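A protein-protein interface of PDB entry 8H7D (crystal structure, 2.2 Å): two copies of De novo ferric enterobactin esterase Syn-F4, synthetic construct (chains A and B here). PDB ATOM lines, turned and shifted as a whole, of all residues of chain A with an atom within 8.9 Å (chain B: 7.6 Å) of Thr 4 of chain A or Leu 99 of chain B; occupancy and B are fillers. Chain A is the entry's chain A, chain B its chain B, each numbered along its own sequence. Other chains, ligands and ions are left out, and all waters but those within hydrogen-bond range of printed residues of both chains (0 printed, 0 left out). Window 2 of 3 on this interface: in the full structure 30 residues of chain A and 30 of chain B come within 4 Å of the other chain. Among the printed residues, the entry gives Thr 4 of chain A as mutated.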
ATOM      1  N   GLY A   3       1.354  21.467  11.483  1.00  0.00           N
ATOM      2  CA  GLY A   3       1.548  22.726  12.262  1.00  0.00           C
ATOM      3  C   GLY A   3       2.883  23.381  11.955  1.00  0.00           C
ATOM      4  O   GLY A   3       3.069  23.942  10.877  1.00  0.00           O
ATOM      5  N   THR A   4       3.799  23.310  12.918  1.00  0.00           N
ATOM      6  CA  THR A   4       5.185  23.793  12.762  1.00  0.00           C
ATOM      7  C   THR A   4       6.235  22.661  12.638  1.00  0.00           C
ATOM      8  O   THR A   4       7.420  22.925  12.367  1.00  0.00           O
ATOM      9  CB  THR A   4       5.568  24.777  13.902  1.00  0.00           C
ATOM     10  OG1 THR A   4       6.767  25.484  13.556  1.00  0.00           O
ATOM     11  CG2 THR A   4       5.755  24.062  15.234  1.00  0.00           C
ATOM     12  N   LEU A   5       5.800  21.414  12.836  1.00  0.00           N
ATOM     13  CA  LEU A   5       6.620  20.239  12.511  1.00  0.00           C
ATOM     14  C   LEU A   5       6.813  20.077  10.989  1.00  0.00           C
ATOM     15  O   LEU A   5       7.694  19.357  10.536  1.00  0.00           O
ATOM     16  CB  LEU A   5       6.003  18.978  13.126  1.00  0.00           C
ATOM     17  CG  LEU A   5       6.922  17.773  13.377  1.00  0.00           C
ATOM     18  CD1 LEU A   5       8.040  18.055  14.381  1.00  0.00           C
ATOM     19  CD2 LEU A   5       6.103  16.589  13.862  1.00  0.00           C
ATOM     20  N   ASN A   6       5.974  20.761  10.219  1.00  0.00           N
ATOM     21  CA  ASN A   6       6.161  20.916   8.782  1.00  0.00           C
ATOM     22  C   ASN A   6       7.383  21.770   8.419  1.00  0.00           C
ATOM     23  O   ASN A   6       8.131  21.429   7.518  1.00  0.00           O
ATOM     24  CB  ASN A   6       4.914  21.555   8.151  1.00  0.00           C
ATOM     25  CG  ASN A   6       3.645  20.745   8.378  1.00  0.00           C
ATOM     26  OD1 ASN A   6       3.417  20.194   9.466  1.00  0.00           O
ATOM     27  ND2 ASN A   6       2.789  20.698   7.357  1.00  0.00           N
ATOM     28  N   GLN A   7       7.524  22.920   9.060  1.00  0.00           N
ATOM     29  CA  GLN A   7       8.657  23.806   8.813  1.00  0.00           C
ATOM     30  C   GLN A   7       9.958  23.088   9.159  1.00  0.00           C
ATOM     31  O   GLN A   7      10.911  23.152   8.389  1.00  0.00           O
ATOM     32  CB  GLN A   7       8.554  25.094   9.609  1.00  0.00           C
ATOM     33  CG  GLN A   7       7.605  26.138   9.022  1.00  0.00           C
ATOM     34  CD  GLN A   7       6.329  26.337   9.850  1.00  0.00           C
ATOM     35  OE1 GLN A   7       6.378  26.368  11.107  1.00  0.00           O
ATOM     36  NE2 GLN A   7       5.178  26.463   9.161  1.00  0.00           N
ATOM     37  N   LEU A   8       9.947  22.363  10.285  1.00  0.00           N
ATOM     38  CA  LEU A   8      11.075  21.538  10.736  1.00  0.00           C
ATOM     39  C   LEU A   8      11.472  20.381   9.803  1.00  0.00           C
ATOM     40  O   LEU A   8      12.677  20.139   9.613  1.00  0.00           O
ATOM     41  CB  LEU A   8      10.827  21.000  12.154  1.00  0.00           C
ATOM     42  CG  LEU A   8      10.719  22.026  13.305  1.00  0.00           C
ATOM     43  CD1 LEU A   8      11.188  21.424  14.624  1.00  0.00           C
ATOM     44  CD2 LEU A   8      11.475  23.328  13.082  1.00  0.00           C
ATOM     45  N   PHE A   9      10.492  19.669   9.254  1.00  0.00           N
ATOM     46  CA  PHE A   9      10.757  18.630   8.279  1.00  0.00           C
ATOM     47  C   PHE A   9      11.447  19.227   7.039  1.00  0.00           C
ATOM     48  O   PHE A   9      12.548  18.808   6.676  1.00  0.00           O
ATOM     49  CB  PHE A   9       9.462  17.901   7.865  1.00  0.00           C
ATOM     50  CG  PHE A   9       9.619  17.070   6.613  1.00  0.00           C
ATOM     51  CD1 PHE A   9      10.429  15.930   6.612  1.00  0.00           C
ATOM     52  CD2 PHE A   9       9.002  17.447   5.414  1.00  0.00           C
ATOM     53  CE1 PHE A   9      10.602  15.180   5.455  1.00  0.00           C
ATOM     54  CE2 PHE A   9       9.178  16.710   4.256  1.00  0.00           C
ATOM     55  CZ  PHE A   9       9.979  15.576   4.274  1.00  0.00           C
ATOM     56  N   HIS A  10      10.773  20.190   6.401  1.00  0.00           N
ATOM     57  CA  HIS A  10      11.235  20.863   5.175  1.00  0.00           C
ATOM     58  C   HIS A  10      12.648  21.389   5.342  1.00  0.00           C
ATOM     59  O   HIS A  10      13.493  21.170   4.474  1.00  0.00           O
ATOM     60  CB  HIS A  10      10.229  21.985   4.825  1.00  0.00           C
ATOM     61  CG  HIS A  10      10.684  22.977   3.801  1.00  0.00           C
ATOM     62  ND1 HIS A  10      10.398  22.854   2.457  1.00  0.00           N
ATOM     63  CD2 HIS A  10      11.321  24.167   3.939  1.00  0.00           C
ATOM     64  CE1 HIS A  10      10.877  23.901   1.807  1.00  0.00           C
ATOM     65  NE2 HIS A  10      11.446  24.708   2.685  1.00  0.00           N
ATOM     66  N   ASN A  11      12.897  22.079   6.443  1.00  0.00           N
ATOM     67  CA  ASN A  11      14.195  22.648   6.726  1.00  0.00           C
ATOM     68  C   ASN A  11      15.313  21.567   6.821  1.00  0.00           C
ATOM     69  O   ASN A  11      16.436  21.745   6.307  1.00  0.00           O
ATOM     70  CB  ASN A  11      14.129  23.405   8.042  1.00  0.00           C
ATOM     71  CG  ASN A  11      13.299  24.674   7.973  1.00  0.00           C
ATOM     72  OD1 ASN A  11      12.918  25.179   6.909  1.00  0.00           O
ATOM     73  ND2 ASN A  11      13.005  25.198   9.142  1.00  0.00           N
ATOM     74  N   LEU A  96      10.287  11.434  10.217  1.00  0.00           N
ATOM     75  CA  LEU A  96       9.789  12.773  10.457  1.00  0.00           C
ATOM     76  C   LEU A  96       8.619  13.084   9.535  1.00  0.00           C
ATOM     77  O   LEU A  96       7.608  13.589   9.996  1.00  0.00           O
ATOM     78  CB  LEU A  96      10.915  13.810  10.313  1.00  0.00           C
ATOM     79  CG  LEU A  96      10.616  15.251  10.725  1.00  0.00           C
ATOM     80  CD1 LEU A  96       9.804  15.355  12.018  1.00  0.00           C
ATOM     81  CD2 LEU A  96      11.919  16.036  10.855  1.00  0.00           C
ATOM     82  N   VAL A 100       4.066  13.739   9.817  1.00  0.00           N
ATOM     83  CA  VAL A 100       3.414  14.941   9.247  1.00  0.00           C
ATOM     84  C   VAL A 100       2.319  14.561   8.236  1.00  0.00           C
ATOM     85  O   VAL A 100       1.897  13.401   8.136  1.00  0.00           O
ATOM     86  CB  VAL A 100       4.458  15.868   8.548  1.00  0.00           C
ATOM     87  CG1 VAL A 100       3.828  17.151   8.017  1.00  0.00           C
ATOM     88  CG2 VAL A 100       5.587  16.242   9.492  1.00  0.00           C
ATOM     89  N   LEU B   5       8.243  12.266  19.117  1.00  0.00           N
ATOM     90  CA  LEU B   5       8.998  13.506  18.914  1.00  0.00           C
ATOM     91  C   LEU B   5      10.287  13.580  19.761  1.00  0.00           C
ATOM     92  O   LEU B   5      11.324  14.052  19.291  1.00  0.00           O
ATOM     93  CB  LEU B   5       8.103  14.719  19.230  1.00  0.00           C
ATOM     94  CG  LEU B   5       8.175  15.873  18.220  1.00  0.00           C
ATOM     95  CD1 LEU B   5       7.440  15.487  16.948  1.00  0.00           C
ATOM     96  CD2 LEU B   5       7.578  17.150  18.788  1.00  0.00           C
ATOM     97  N   LEU B  93      17.711  22.170  16.024  1.00  0.00           N
ATOM     98  CA  LEU B  93      17.639  21.326  17.241  1.00  0.00           C
ATOM     99  C   LEU B  93      16.930  22.084  18.359  1.00  0.00           C
ATOM    100  O   LEU B  93      16.127  21.489  19.076  1.00  0.00           O
ATOM    101  CB  LEU B  93      19.011  20.856  17.741  1.00  0.00           C
ATOM    102  CG  LEU B  93      19.565  19.581  17.107  1.00  0.00           C
ATOM    103  CD1 LEU B  93      20.999  19.356  17.578  1.00  0.00           C
ATOM    104  CD2 LEU B  93      18.728  18.353  17.396  1.00  0.00           C
ATOM    105  N   ALA B  94      17.242  23.383  18.483  1.00  0.00           N
ATOM    106  CA  ALA B  94      16.607  24.269  19.481  1.00  0.00           C
ATOM    107  C   ALA B  94      15.099  24.377  19.252  1.00  0.00           C
ATOM    108  O   ALA B  94      14.321  24.379  20.208  1.00  0.00           O
ATOM    109  CB  ALA B  94      17.258  25.628  19.512  1.00  0.00           C
ATOM    110  N   GLN B  95      14.692  24.386  17.997  1.00  0.00           N
ATOM    111  CA  GLN B  95      13.280  24.385  17.645  1.00  0.00           C
ATOM    112  C   GLN B  95      12.607  23.078  18.038  1.00  0.00           C
ATOM    113  O   GLN B  95      11.530  23.080  18.632  1.00  0.00           O
ATOM    114  CB  GLN B  95      13.118  24.680  16.161  1.00  0.00           C
ATOM    115  CG  GLN B  95      13.194  26.165  15.851  1.00  0.00           C
ATOM    116  CD  GLN B  95      13.649  26.491  14.429  1.00  0.00           C
ATOM    117  OE1 GLN B  95      13.643  25.644  13.536  1.00  0.00           O
ATOM    118  NE2 GLN B  95      14.030  27.739  14.213  1.00  0.00           N
ATOM    119  N   LEU B  96      13.262  21.962  17.727  1.00  0.00           N
ATOM    120  CA  LEU B  96      12.804  20.663  18.197  1.00  0.00           C
ATOM    121  C   LEU B  96      12.656  20.650  19.722  1.00  0.00           C
ATOM    122  O   LEU B  96      11.606  20.314  20.213  1.00  0.00           O
ATOM    123  CB  LEU B  96      13.724  19.532  17.738  1.00  0.00           C
ATOM    124  CG  LEU B  96      13.349  18.769  16.463  1.00  0.00           C
ATOM    125  CD1 LEU B  96      14.308  17.596  16.286  1.00  0.00           C
ATOM    126  CD2 LEU B  96      11.909  18.231  16.464  1.00  0.00           C
ATOM    127  N   ASP B  97      13.727  21.013  20.429  1.00  0.00           N
ATOM    128  CA  ASP B  97      13.776  21.154  21.898  1.00  0.00           C
ATOM    129  C   ASP B  97      12.516  21.854  22.419  1.00  0.00           C
ATOM    130  O   ASP B  97      11.804  21.301  23.237  1.00  0.00           O
ATOM    131  CB  ASP B  97      15.037  21.967  22.315  1.00  0.00           C
ATOM    132  CG  ASP B  97      15.677  21.497  23.629  1.00  0.00           C
ATOM    133  OD1 ASP B  97      15.090  20.700  24.376  1.00  0.00           O
ATOM    134  OD2 ASP B  97      16.821  21.934  23.902  1.00  0.00           O
ATOM    135  N   ASN B  98      12.239  23.048  21.894  1.00  0.00           N
ATOM    136  CA  ASN B  98      11.020  23.823  22.212  1.00  0.00           C
ATOM    137  C   ASN B  98       9.709  23.076  21.924  1.00  0.00           C
ATOM    138  O   ASN B  98       8.792  23.073  22.751  1.00  0.00           O
ATOM    139  CB  ASN B  98      11.011  25.153  21.440  1.00  0.00           C
ATOM    140  CG  ASN B  98      11.871  26.230  22.085  1.00  0.00           C
ATOM    141  OD1 ASN B  98      12.446  26.039  23.160  1.00  0.00           O
ATOM    142  ND2 ASN B  98      11.951  27.392  21.420  1.00  0.00           N
ATOM    143  N   LEU B  99       9.634  22.454  20.755  1.00  0.00           N
ATOM    144  CA  LEU B  99       8.414  21.787  20.307  1.00  0.00           C
ATOM    145  C   LEU B  99       8.077  20.499  21.080  1.00  0.00           C
ATOM    146  O   LEU B  99       6.884  20.199  21.323  1.00  0.00           O
ATOM    147  CB  LEU B  99       8.509  21.514  18.813  1.00  0.00           C
ATOM    148  CG  LEU B  99       7.255  20.949  18.137  1.00  0.00           C
ATOM    149  CD1 LEU B  99       6.168  22.013  18.049  1.00  0.00           C
ATOM    150  CD2 LEU B  99       7.593  20.406  16.760  1.00  0.00           C
ATOM    151  N   VAL B 100       9.102  19.739  21.463  1.00  0.00           N
ATOM    152  CA  VAL B 100       8.874  18.496  22.214  1.00  0.00           C
ATOM    153  C   VAL B 100       8.241  18.753  23.599  1.00  0.00           C
ATOM    154  O   VAL B 100       7.177  18.216  23.906  1.00  0.00           O
ATOM    155  CB  VAL B 100      10.130  17.578  22.307  1.00  0.00           C
ATOM    156  CG1 VAL B 100      10.587  17.143  20.930  1.00  0.00           C
ATOM    157  CG2 VAL B 100      11.295  18.206  23.042  1.00  0.00           C
ATOM    158  N   HIS B 101       8.868  19.620  24.383  1.00  0.00           N
ATOM    159  CA  HIS B 101       8.499  19.854  25.782  1.00  0.00           C
ATOM    160  C   HIS B 101       7.208  20.674  25.988  1.00  0.00           C
ATOM    161  O   HIS B 101       6.553  20.549  27.031  1.00  0.00           O
ATOM    162  CB  HIS B 101       9.657  20.541  26.497  1.00  0.00           C
ATOM    163  CG  HIS B 101      10.887  19.706  26.540  1.00  0.00           C
ATOM    164  ND1 HIS B 101      12.082  20.107  25.991  1.00  0.00           N
ATOM    165  CD2 HIS B 101      11.096  18.469  27.034  1.00  0.00           C
ATOM    166  CE1 HIS B 101      12.980  19.153  26.154  1.00  0.00           C
ATOM    167  NE2 HIS B 101      12.405  18.147  26.783  1.00  0.00           N
ATOM    168  N   ARG B 102       6.869  21.508  25.001  1.00  0.00           N
ATOM    169  CA  ARG B 102       5.684  22.374  25.008  1.00  0.00           C
ATOM    170  C   ARG B 102       4.443  21.737  25.635  1.00  0.00           C
ATOM    171  O   ARG B 102       3.674  22.401  26.327  1.00  0.00           O
ATOM    172  CB  ARG B 102       5.384  22.794  23.566  1.00  0.00           C
ATOM    173  CG  ARG B 102       4.024  23.443  23.321  1.00  0.00           C
ATOM    174  CD  ARG B 102       2.893  22.444  23.042  1.00  0.00           C
ATOM    175  NE  ARG B 102       3.227  21.515  21.967  1.00  0.00           N
ATOM    176  CZ  ARG B 102       3.230  21.826  20.672  1.00  0.00           C
ATOM    177  NH1 ARG B 102       2.913  23.055  20.250  1.00  0.00           N
ATOM    178  NH2 ARG B 102       3.558  20.896  19.783  1.00  0.00           N
ATOM    179  OXT ARG B 102       4.142  20.563  25.430  1.00  0.00           O
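OE1 of Gln 7 of chain A is in hydrogen-bond range of OG1 of Thr 4 of chain A, at 2.6 Å.
CD1 of Leu 99 of chain B touches CG2 of Thr 4 of chain A (3.5 Å).
Leu 5 of chain A touches Leu 5 of chain B (CD2 to CD1, 3.5 Å).
Leu 5 of chain A touches Leu 99 of chain B (CD1 to CD2, 3.4 Å).
Gln 95 of chain B touches Leu 8 of chain A (OE1 to CD2, 3.2 Å).
Leu 8 of chain A touches Leu 96 of chain B (CD1 to CD2, 3.8 Å).
No residue of chain B comes within 4 Å of Gly 3 of chain A.
Printed residues of chain B within 4 Å of Leu 5 of chain A: Leu 5 (3.5 Å) and Leu 99 (3.4 Å).
Of the printed residues of chain B, Leu 8 of chain A touches Gln 95 (3.2 Å) and Leu 96 (3.8 Å).
Of the printed residues of chain A, Leu 5 of chain B touches Leu 5 (3.5 Å).
Printed residues of chain A within 4 Å of Gln 95 of chain B: Leu 8 (3.2 Å).
Of the printed residues of chain A, Leu 96 of chain B touches Leu 8 (3.8 Å).
Leu 99 of chain B touches just these residues of chain A: Thr 4 (3.5 Å) and Leu 5 (3.4 Å).
Of the 11 printed residues of chain A, 3 touch a printed residue of chain B.
Printed residues of chain A that touch a printed residue of chain B: Thr 4, Leu 5 and Leu 8.
Of the 11 printed residues of chain B, 4 touch a printed residue of chain A.
Hydrophobic or aromatic side chains of chain B that line the printed part of chain A: Leu 5, Leu 96 and Leu 99.
Among the printed residues, 5 pairs touch across the chains.
Among the printed residues, no Asp or Glu carboxylate lies within 4 Å of a Lys or Arg side-chain nitrogen of the other chain.
Leu 5 of chain B touches its own counterpart, Leu 5 of chain A.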
